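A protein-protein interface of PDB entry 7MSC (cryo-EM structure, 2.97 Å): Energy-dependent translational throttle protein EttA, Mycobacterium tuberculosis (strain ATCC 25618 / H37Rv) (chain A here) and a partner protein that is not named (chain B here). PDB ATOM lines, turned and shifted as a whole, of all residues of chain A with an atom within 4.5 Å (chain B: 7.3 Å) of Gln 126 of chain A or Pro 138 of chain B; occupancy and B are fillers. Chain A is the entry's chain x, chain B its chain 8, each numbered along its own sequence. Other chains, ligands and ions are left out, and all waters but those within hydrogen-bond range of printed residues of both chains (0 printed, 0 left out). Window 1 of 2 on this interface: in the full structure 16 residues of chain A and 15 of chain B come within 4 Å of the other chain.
Along chain B the printed residues that touch a printed residue of chain A span positions 60 to 141. Of the 10 printed residues of chain A, 7 touch a printed residue of chain B. Hydrophobic or aromatic side chains of chain A that line the printed part of chain B: Met 122 and Trp 135. Among the printed residues, 12 pairs touch across the chains. Among the printed residues, Asp or Glu carboxylates within 4 Å of a Lys or Arg side-chain nitrogen of the other chain: Glu 127 of chain A with Arg 60 of chain B (3.5 Å), Glu 127 of chain A with Lys 141 of chain B (3.6 Å) and Asp 130 of chain A with Arg 60 of chain B (3.6 Å).
Of the printed residues of chain B, Gln 126 of chain A touches Met 137 (2.8 Å), Pro 138 (2.7 Å) and Pro 140 (3.9999 Å). Pro 138 of chain B touches just one residue of chain A: Gln 126 (2.7 Å). Of the printed residues of chain A, Arg 60 of chain B touches Glu 127 (3.2 Å) and Asp 130 (3.6 Å). Printed residues of chain B within 4 Å of Glu 127 of chain A: Arg 60 (3.2 Å) and Lys 141 (3.3 Å). Of the printed residues of chain B, Trp 135 of chain A touches Ala 128 and Gly 132. Ala 113 of chain B touches none of the printed residues of chain A. The nearest printed residue of chain B that does not touch Gln 126 of chain A is Asn 139 of chain B (4.5 Å).
O of Gly 123 of chain A sits at hydrogen-bond distance from NZ of Lys 141 of chain B (3.1 Å). The side-chain amide nitrogen of Gln 126 of chain A is in hydrogen-bond range of the side-chain sulfur of Met 137 of chain B. The side-chain amide nitrogen (NE2) of Gln 126 of chain A sits at hydrogen-bond distance from the backbone carbonyl oxygen (O) of Pro 138 of chain B. The side-chain carboxylate (OE1) of Glu 127 of chain A lies within salt-bridge range of the guanidinium group (NH2) of Arg 60 of chain B, 3.5 Å away. The side-chain carboxylate (OE2) of Glu 127 of chain A is in salt-bridge range of the side-chain amino group (NZ) of Lys 141 of chain B. The side-chain carboxylate of Asp 130 of chain A lies within salt-bridge range of the guanidinium group of Arg 60 of chain B, at 3.6 Å.
O of Met 122 of chain A lies close to OE1 of Gln 126 of chain A (3.5 Å). The indole nitrogen (NE1) of Trp 135 of chain A sits at hydrogen-bond distance from the backbone carbonyl oxygen (O) of Leu 129 of chain A (3.0 Å). The backbone carbonyl oxygen (O) of Leu 131 of chain B is in hydrogen-bond range of the backbone NH (N) of Met 137 of chain B (3.2 Å). The side-chain amide oxygen of Asn 139 of chain B sits at hydrogen-bond distance from the side-chain amino group of Lys 141 of chain B (3.3 Å).
Among the printed residues, merely in contact across the chains: Trp 135 of chain A with Ala 128 of chain B (3.2 Å), Trp 135 of chain A with Gly 132 of chain B (3.6 Å), Met 122 of chain A with Met 121 of chain B (3.8 Å), Gly 123 of chain A with Pro 140 of chain B (3.9 Å), Arg 124 of chain A with Lys 141 of chain B (3.9 Å) and Gln 126 of chain A with Pro 140 of chain B (3.9999 Å).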
ATOM      1  N   MET A 122      12.372   1.866  -0.831  1.00  0.00           N
ATOM      2  CA  MET A 122      12.606   3.257  -0.483  1.00  0.00           C
ATOM      3  C   MET A 122      11.357   4.099  -0.676  1.00  0.00           C
ATOM      4  O   MET A 122      11.420   5.325  -0.548  1.00  0.00           O
ATOM      5  CB  MET A 122      13.783   3.827  -1.284  1.00  0.00           C
ATOM      6  CG  MET A 122      13.631   3.851  -2.799  1.00  0.00           C
ATOM      7  SD  MET A 122      12.861   5.331  -3.490  1.00  0.00           S
ATOM      8  CE  MET A 122      14.147   6.538  -3.181  1.00  0.00           C
ATOM      9  N   GLY A 123      10.229   3.465  -0.980  1.00  0.00           N
ATOM     10  CA  GLY A 123       8.969   4.165  -1.089  1.00  0.00           C
ATOM     11  C   GLY A 123       8.146   4.109   0.180  1.00  0.00           C
ATOM     12  O   GLY A 123       7.709   5.149   0.682  1.00  0.00           O
ATOM     13  N   ARG A 124       7.927   2.908   0.722  1.00  0.00           N
ATOM     14  CA  ARG A 124       7.117   2.791   1.928  1.00  0.00           C
ATOM     15  C   ARG A 124       7.869   3.208   3.185  1.00  0.00           C
ATOM     16  O   ARG A 124       7.238   3.378   4.234  1.00  0.00           O
ATOM     17  CB  ARG A 124       6.571   1.366   2.077  1.00  0.00           C
ATOM     18  CG  ARG A 124       7.598   0.282   2.313  1.00  0.00           C
ATOM     19  CD  ARG A 124       6.905  -1.069   2.424  1.00  0.00           C
ATOM     20  NE  ARG A 124       7.845  -2.175   2.576  1.00  0.00           N
ATOM     21  CZ  ARG A 124       8.285  -2.624   3.745  1.00  0.00           C
ATOM     22  NH1 ARG A 124       7.867  -2.063   4.872  1.00  0.00           N
ATOM     23  NH2 ARG A 124       9.139  -3.637   3.789  1.00  0.00           N
ATOM     24  N   LEU A 125       9.191   3.373   3.111  1.00  0.00           N
ATOM     25  CA  LEU A 125       9.885   4.138   4.139  1.00  0.00           C
ATOM     26  C   LEU A 125       9.549   5.613   4.020  1.00  0.00           C
ATOM     27  O   LEU A 125       9.314   6.290   5.025  1.00  0.00           O
ATOM     28  CB  LEU A 125      11.392   3.949   4.026  1.00  0.00           C
ATOM     29  CG  LEU A 125      11.978   2.570   4.278  1.00  0.00           C
ATOM     30  CD1 LEU A 125      13.466   2.641   4.031  1.00  0.00           C
ATOM     31  CD2 LEU A 125      11.676   2.083   5.676  1.00  0.00           C
ATOM     32  N   GLN A 126       9.519   6.123   2.789  1.00  0.00           N
ATOM     33  CA  GLN A 126       9.267   7.536   2.553  1.00  0.00           C
ATOM     34  C   GLN A 126       7.816   7.907   2.835  1.00  0.00           C
ATOM     35  O   GLN A 126       7.524   9.078   3.094  1.00  0.00           O
ATOM     36  CB  GLN A 126       9.669   7.866   1.116  1.00  0.00           C
ATOM     37  CG  GLN A 126       9.803   9.331   0.781  1.00  0.00           C
ATOM     38  CD  GLN A 126      10.337   9.531  -0.623  1.00  0.00           C
ATOM     39  OE1 GLN A 126      10.522   8.572  -1.367  1.00  0.00           O
ATOM     40  NE2 GLN A 126      10.606  10.778  -0.988  1.00  0.00           N
ATOM     41  N   GLU A 127       6.906   6.931   2.818  1.00  0.00           N
ATOM     42  CA  GLU A 127       5.559   7.139   3.330  1.00  0.00           C
ATOM     43  C   GLU A 127       5.477   7.062   4.848  1.00  0.00           C
ATOM     44  O   GLU A 127       4.421   7.372   5.406  1.00  0.00           O
ATOM     45  CB  GLU A 127       4.577   6.126   2.730  1.00  0.00           C
ATOM     46  CG  GLU A 127       4.174   6.401   1.288  1.00  0.00           C
ATOM     47  CD  GLU A 127       3.123   5.424   0.783  1.00  0.00           C
ATOM     48  OE1 GLU A 127       2.861   4.417   1.476  1.00  0.00           O
ATOM     49  OE2 GLU A 127       2.529   5.685  -0.283  1.00  0.00           O
ATOM     50  N   GLU A 128       6.544   6.646   5.529  1.00  0.00           N
ATOM     51  CA  GLU A 128       6.597   6.685   6.984  1.00  0.00           C
ATOM     52  C   GLU A 128       7.569   7.745   7.481  1.00  0.00           C
ATOM     53  O   GLU A 128       8.167   7.600   8.548  1.00  0.00           O
ATOM     54  CB  GLU A 128       6.958   5.318   7.558  1.00  0.00           C
ATOM     55  CG  GLU A 128       5.862   4.286   7.393  1.00  0.00           C
ATOM     56  CD  GLU A 128       6.227   2.953   8.004  1.00  0.00           C
ATOM     57  OE1 GLU A 128       7.382   2.797   8.450  1.00  0.00           O
ATOM     58  OE2 GLU A 128       5.359   2.058   8.040  1.00  0.00           O
ATOM     59  N   LEU A 129       7.745   8.810   6.705  1.00  0.00           N
ATOM     60  CA  LEU A 129       8.523   9.958   7.131  1.00  0.00           C
ATOM     61  C   LEU A 129       7.764  11.265   6.976  1.00  0.00           C
ATOM     62  O   LEU A 129       8.329  12.324   7.262  1.00  0.00           O
ATOM     63  CB  LEU A 129       9.844  10.048   6.350  1.00  0.00           C
ATOM     64  CG  LEU A 129      10.845   8.905   6.519  1.00  0.00           C
ATOM     65  CD1 LEU A 129      12.062   9.129   5.645  1.00  0.00           C
ATOM     66  CD2 LEU A 129      11.250   8.737   7.964  1.00  0.00           C
ATOM     67  N   ASP A 130       6.511  11.227   6.533  1.00  0.00           N
ATOM     68  CA  ASP A 130       5.717  12.435   6.346  1.00  0.00           C
ATOM     69  C   ASP A 130       4.591  12.595   7.356  1.00  0.00           C
ATOM     70  O   ASP A 130       4.301  13.719   7.767  1.00  0.00           O
ATOM     71  CB  ASP A 130       5.152  12.480   4.919  1.00  0.00           C
ATOM     72  CG  ASP A 130       4.364  11.233   4.549  1.00  0.00           C
ATOM     73  OD1 ASP A 130       4.286  10.290   5.364  1.00  0.00           O
ATOM     74  OD2 ASP A 130       3.830  11.189   3.420  1.00  0.00           O
ATOM     75  N   TRP A 135      12.033  13.843   9.243  1.00  0.00           N
ATOM     76  CA  TRP A 135      13.115  14.381   8.428  1.00  0.00           C
ATOM     77  C   TRP A 135      14.066  15.247   9.237  1.00  0.00           C
ATOM     78  O   TRP A 135      15.222  15.420   8.837  1.00  0.00           O
ATOM     79  CB  TRP A 135      12.559  15.196   7.260  1.00  0.00           C
ATOM     80  CG  TRP A 135      11.816  14.377   6.261  1.00  0.00           C
ATOM     81  CD1 TRP A 135      10.466  14.264   6.133  1.00  0.00           C
ATOM     82  CD2 TRP A 135      12.385  13.537   5.257  1.00  0.00           C
ATOM     83  NE1 TRP A 135      10.156  13.410   5.106  1.00  0.00           N
ATOM     84  CE2 TRP A 135      11.320  12.949   4.551  1.00  0.00           C
ATOM     85  CE3 TRP A 135      13.693  13.230   4.879  1.00  0.00           C
ATOM     86  CZ2 TRP A 135      11.523  12.071   3.490  1.00  0.00           C
ATOM     87  CZ3 TRP A 135      13.893  12.353   3.829  1.00  0.00           C
ATOM     88  CH2 TRP A 135      12.815  11.786   3.145  1.00  0.00           C
ATOM     89  N   ARG B  60      -3.960   7.973   0.108  1.00  0.00           N
ATOM     90  CA  ARG B  60      -2.874   8.656  -0.578  1.00  0.00           C
ATOM     91  C   ARG B  60      -2.838   8.207  -2.026  1.00  0.00           C
ATOM     92  O   ARG B  60      -2.787   7.006  -2.304  1.00  0.00           O
ATOM     93  CB  ARG B  60      -1.526   8.371   0.087  1.00  0.00           C
ATOM     94  CG  ARG B  60      -0.361   9.101  -0.548  1.00  0.00           C
ATOM     95  CD  ARG B  60       0.946   8.775   0.157  1.00  0.00           C
ATOM     96  NE  ARG B  60       0.971   9.260   1.533  1.00  0.00           N
ATOM     97  CZ  ARG B  60       0.997   8.474   2.605  1.00  0.00           C
ATOM     98  NH1 ARG B  60       1.020   9.004   3.820  1.00  0.00           N
ATOM     99  NH2 ARG B  60       0.995   7.157   2.464  1.00  0.00           N
ATOM    100  N   PHE B  78      15.921  15.557 -12.111  1.00  0.00           N
ATOM    101  CA  PHE B  78      17.244  14.994 -11.850  1.00  0.00           C
ATOM    102  C   PHE B  78      17.515  13.928 -12.903  1.00  0.00           C
ATOM    103  O   PHE B  78      16.977  12.821 -12.833  1.00  0.00           O
ATOM    104  CB  PHE B  78      17.323  14.403 -10.449  1.00  0.00           C
ATOM    105  CG  PHE B  78      17.264  15.419  -9.355  1.00  0.00           C
ATOM    106  CD1 PHE B  78      18.394  16.136  -8.996  1.00  0.00           C
ATOM    107  CD2 PHE B  78      16.085  15.645  -8.669  1.00  0.00           C
ATOM    108  CE1 PHE B  78      18.344  17.065  -7.976  1.00  0.00           C
ATOM    109  CE2 PHE B  78      16.028  16.574  -7.650  1.00  0.00           C
ATOM    110  CZ  PHE B  78      17.159  17.283  -7.304  1.00  0.00           C
ATOM    111  N   PHE B 111      10.377  25.094  -7.694  1.00  0.00           N
ATOM    112  CA  PHE B 111       9.776  24.061  -8.526  1.00  0.00           C
ATOM    113  C   PHE B 111       8.663  23.411  -7.721  1.00  0.00           C
ATOM    114  O   PHE B 111       8.515  23.654  -6.522  1.00  0.00           O
ATOM    115  CB  PHE B 111      10.815  23.039  -9.013  1.00  0.00           C
ATOM    116  CG  PHE B 111      11.510  22.283  -7.912  1.00  0.00           C
ATOM    117  CD1 PHE B 111      12.638  22.806  -7.297  1.00  0.00           C
ATOM    118  CD2 PHE B 111      11.074  21.022  -7.537  1.00  0.00           C
ATOM    119  CE1 PHE B 111      13.287  22.108  -6.298  1.00  0.00           C
ATOM    120  CE2 PHE B 111      11.723  20.313  -6.547  1.00  0.00           C
ATOM    121  CZ  PHE B 111      12.829  20.859  -5.922  1.00  0.00           C
ATOM    122  N   ALA B 113       7.190  19.715  -8.551  1.00  0.00           N
ATOM    123  CA  ALA B 113       7.342  18.276  -8.412  1.00  0.00           C
ATOM    124  C   ALA B 113       8.647  17.841  -9.059  1.00  0.00           C
ATOM    125  O   ALA B 113       9.024  18.351 -10.118  1.00  0.00           O
ATOM    126  CB  ALA B 113       6.166  17.528  -9.045  1.00  0.00           C
ATOM    127  N   ALA B 114       9.328  16.898  -8.420  1.00  0.00           N
ATOM    128  CA  ALA B 114      10.614  16.414  -8.889  1.00  0.00           C
ATOM    129  C   ALA B 114      10.442  15.118  -9.668  1.00  0.00           C
ATOM    130  O   ALA B 114       9.552  14.315  -9.386  1.00  0.00           O
ATOM    131  CB  ALA B 114      11.573  16.194  -7.719  1.00  0.00           C
ATOM    132  N   ILE B 115      11.300  14.931 -10.668  1.00  0.00           N
ATOM    133  CA  ILE B 115      11.318  13.730 -11.495  1.00  0.00           C
ATOM    134  C   ILE B 115      12.755  13.239 -11.577  1.00  0.00           C
ATOM    135  O   ILE B 115      13.651  13.999 -11.956  1.00  0.00           O
ATOM    136  CB  ILE B 115      10.747  13.992 -12.903  1.00  0.00           C
ATOM    137  CG1 ILE B 115       9.248  14.287 -12.832  1.00  0.00           C
ATOM    138  CG2 ILE B 115      11.004  12.812 -13.824  1.00  0.00           C
ATOM    139  CD1 ILE B 115       8.657  14.778 -14.128  1.00  0.00           C
ATOM    140  N   ALA B 116      12.976  11.978 -11.217  1.00  0.00           N
ATOM    141  CA  ALA B 116      14.325  11.436 -11.216  1.00  0.00           C
ATOM    142  C   ALA B 116      14.301   9.968 -11.609  1.00  0.00           C
ATOM    143  O   ALA B 116      13.305   9.269 -11.411  1.00  0.00           O
ATOM    144  CB  ALA B 116      14.986  11.596  -9.844  1.00  0.00           C
ATOM    145  N   MET B 121      18.464   9.056  -7.694  1.00  0.00           N
ATOM    146  CA  MET B 121      17.935   9.169  -6.337  1.00  0.00           C
ATOM    147  C   MET B 121      18.953   8.831  -5.258  1.00  0.00           C
ATOM    148  O   MET B 121      18.648   9.006  -4.074  1.00  0.00           O
ATOM    149  CB  MET B 121      16.709   8.270  -6.171  1.00  0.00           C
ATOM    150  CG  MET B 121      15.482   8.743  -6.927  1.00  0.00           C
ATOM    151  SD  MET B 121      14.946  10.370  -6.364  1.00  0.00           S
ATOM    152  CE  MET B 121      14.393   9.995  -4.703  1.00  0.00           C
ATOM    153  N   VAL B 124      19.952  12.520  -4.219  1.00  0.00           N
ATOM    154  CA  VAL B 124      18.892  13.486  -3.943  1.00  0.00           C
ATOM    155  C   VAL B 124      18.324  13.289  -2.542  1.00  0.00           C
ATOM    156  O   VAL B 124      18.025  14.262  -1.843  1.00  0.00           O
ATOM    157  CB  VAL B 124      17.801  13.364  -5.027  1.00  0.00           C
ATOM    158  CG1 VAL B 124      16.642  14.314  -4.769  1.00  0.00           C
ATOM    159  CG2 VAL B 124      18.396  13.618  -6.394  1.00  0.00           C
ATOM    160  N   GLY B 125      18.210  12.031  -2.108  1.00  0.00           N
ATOM    161  CA  GLY B 125      17.624  11.704  -0.819  1.00  0.00           C
ATOM    162  C   GLY B 125      18.427  12.171   0.378  1.00  0.00           C
ATOM    163  O   GLY B 125      17.859  12.332   1.462  1.00  0.00           O
ATOM    164  N   ALA B 128      17.189  15.570   0.648  1.00  0.00           N
ATOM    165  CA  ALA B 128      15.766  15.526   1.000  1.00  0.00           C
ATOM    166  C   ALA B 128      15.475  15.849   2.480  1.00  0.00           C
ATOM    167  O   ALA B 128      14.304  15.679   2.837  1.00  0.00           O
ATOM    168  CB  ALA B 128      15.185  14.157   0.654  1.00  0.00           C
ATOM    169  N   LEU B 131      13.717  18.836   1.394  1.00  0.00           N
ATOM    170  CA  LEU B 131      12.653  18.493   0.462  1.00  0.00           C
ATOM    171  C   LEU B 131      11.625  17.555   1.073  1.00  0.00           C
ATOM    172  O   LEU B 131      10.629  17.233   0.416  1.00  0.00           O
ATOM    173  CB  LEU B 131      13.239  17.847  -0.794  1.00  0.00           C
ATOM    174  CG  LEU B 131      14.103  18.756  -1.658  1.00  0.00           C
ATOM    175  CD1 LEU B 131      14.762  17.959  -2.764  1.00  0.00           C
ATOM    176  CD2 LEU B 131      13.251  19.868  -2.236  1.00  0.00           C
ATOM    177  N   GLY B 132      11.849  17.109   2.304  1.00  0.00           N
ATOM    178  CA  GLY B 132      10.996  16.142   2.953  1.00  0.00           C
ATOM    179  C   GLY B 132       9.621  16.658   3.328  1.00  0.00           C
ATOM    180  O   GLY B 132       8.611  16.252   2.745  1.00  0.00           O
ATOM    181  N   GLY B 135       6.873  18.298   0.601  1.00  0.00           N
ATOM    182  CA  GLY B 135       6.169  17.570  -0.432  1.00  0.00           C
ATOM    183  C   GLY B 135       6.792  17.648  -1.805  1.00  0.00           C
ATOM    184  O   GLY B 135       6.189  17.166  -2.771  1.00  0.00           O
ATOM    185  N   LEU B 136       7.972  18.242  -1.925  1.00  0.00           N
ATOM    186  CA  LEU B 136       8.697  18.309  -3.183  1.00  0.00           C
ATOM    187  C   LEU B 136       9.614  17.112  -3.378  1.00  0.00           C
ATOM    188  O   LEU B 136      10.307  17.036  -4.397  1.00  0.00           O
ATOM    189  CB  LEU B 136       9.506  19.611  -3.257  1.00  0.00           C
ATOM    190  CG  LEU B 136       8.838  20.929  -3.684  1.00  0.00           C
ATOM    191  CD1 LEU B 136       7.849  21.476  -2.663  1.00  0.00           C
ATOM    192  CD2 LEU B 136       9.902  21.979  -3.957  1.00  0.00           C
ATOM    193  N   MET B 137       9.629  16.187  -2.420  1.00  0.00           N
ATOM    194  CA  MET B 137      10.433  14.982  -2.525  1.00  0.00           C
ATOM    195  C   MET B 137       9.879  14.048  -3.602  1.00  0.00           C
ATOM    196  O   MET B 137       8.672  14.024  -3.856  1.00  0.00           O
ATOM    197  CB  MET B 137      10.487  14.269  -1.172  1.00  0.00           C
ATOM    198  CG  MET B 137       9.125  13.939  -0.544  1.00  0.00           C
ATOM    199  SD  MET B 137       8.350  12.374  -1.020  1.00  0.00           S
ATOM    200  CE  MET B 137       6.614  12.736  -0.734  1.00  0.00           C
ATOM    201  N   PRO B 138      10.747  13.290  -4.268  1.00  0.00           N
ATOM    202  CA  PRO B 138      10.270  12.347  -5.284  1.00  0.00           C
ATOM    203  C   PRO B 138       9.643  11.118  -4.647  1.00  0.00           C
ATOM    204  O   PRO B 138      10.176  10.547  -3.693  1.00  0.00           O
ATOM    205  CB  PRO B 138      11.543  11.989  -6.057  1.00  0.00           C
ATOM    206  CG  PRO B 138      12.505  13.098  -5.753  1.00  0.00           C
ATOM    207  CD  PRO B 138      12.204  13.485  -4.346  1.00  0.00           C
ATOM    208  N   ASN B 139       8.503  10.710  -5.199  1.00  0.00           N
ATOM    209  CA  ASN B 139       7.687   9.619  -4.678  1.00  0.00           C
ATOM    210  C   ASN B 139       7.510   8.589  -5.786  1.00  0.00           C
ATOM    211  O   ASN B 139       6.932   8.920  -6.837  1.00  0.00           O
ATOM    212  CB  ASN B 139       6.333  10.160  -4.211  1.00  0.00           C
ATOM    213  CG  ASN B 139       5.560   9.176  -3.365  1.00  0.00           C
ATOM    214  OD1 ASN B 139       6.004   8.059  -3.123  1.00  0.00           O
ATOM    215  ND2 ASN B 139       4.393   9.597  -2.895  1.00  0.00           N
ATOM    216  N   PRO B 140       7.989   7.349  -5.623  1.00  0.00           N
ATOM    217  CA  PRO B 140       7.983   6.401  -6.749  1.00  0.00           C
ATOM    218  C   PRO B 140       6.614   5.862  -7.122  1.00  0.00           C
ATOM    219  O   PRO B 140       6.489   5.254  -8.193  1.00  0.00           O
ATOM    220  CB  PRO B 140       8.896   5.272  -6.258  1.00  0.00           C
ATOM    221  CG  PRO B 140       8.825   5.347  -4.785  1.00  0.00           C
ATOM    222  CD  PRO B 140       8.693   6.801  -4.452  1.00  0.00           C
ATOM    223  N   LYS B 141       5.590   6.050  -6.290  1.00  0.00           N
ATOM    224  CA  LYS B 141       4.265   5.557  -6.648  1.00  0.00           C
ATOM    225  C   LYS B 141       3.587   6.449  -7.676  1.00  0.00           C
ATOM    226  O   LYS B 141       2.803   5.957  -8.494  1.00  0.00           O
ATOM    227  CB  LYS B 141       3.374   5.440  -5.411  1.00  0.00           C
ATOM    228  CG  LYS B 141       3.472   4.116  -4.670  1.00  0.00           C
ATOM    229  CD  LYS B 141       4.714   4.048  -3.813  1.00  0.00           C
ATOM    230  CE  LYS B 141       4.634   5.088  -2.721  1.00  0.00           C
ATOM    231  NZ  LYS B 141       5.788   5.057  -1.792  1.00  0.00           N
ATOM    232  N   THR B 142       3.879   7.747  -7.659  1.00  0.00           N
ATOM    233  CA  THR B 142       3.290   8.694  -8.593  1.00  0.00           C
ATOM    234  C   THR B 142       4.107   8.845  -9.870  1.00  0.00           C
ATOM    235  O   THR B 142       4.034   9.892 -10.524  1.00  0.00           O
ATOM    236  CB  THR B 142       3.110  10.054  -7.918  1.00  0.00           C
ATOM    237  OG1 THR B 142       4.385  10.550  -7.495  1.00  0.00           O
ATOM    238  CG2 THR B 142       2.201   9.925  -6.713  1.00  0.00           C
ATOM    239  N   THR B 144       7.223   9.340 -10.377  1.00  0.00           N
ATOM    240  CA  THR B 144       8.318  10.297 -10.381  1.00  0.00           C
ATOM    241  C   THR B 144       9.680   9.637 -10.244  1.00  0.00           C
ATOM    242  O   THR B 144      10.688  10.254 -10.604  1.00  0.00           O
ATOM    243  CB  THR B 144       8.128  11.319  -9.263  1.00  0.00           C
ATOM    244  OG1 THR B 144       8.201  10.658  -7.997  1.00  0.00           O
ATOM    245  CG2 THR B 144       6.774  11.991  -9.395  1.00  0.00           C
ATOM    246  N   VAL B 145       9.741   8.413  -9.732  1.00  0.00           N
ATOM    247  CA  VAL B 145      10.988   7.657  -9.643  1.00  0.00           C
ATOM    248  C   VAL B 145      10.804   6.426 -10.522  1.00  0.00           C
ATOM    249  O   VAL B 145      10.252   5.408 -10.093  1.00  0.00           O
ATOM    250  CB  VAL B 145      11.347   7.277  -8.205  1.00  0.00           C
ATOM    251  CG1 VAL B 145      12.667   6.510  -8.161  1.00  0.00           C
ATOM    252  CG2 VAL B 145      11.410   8.509  -7.330  1.00  0.00           C
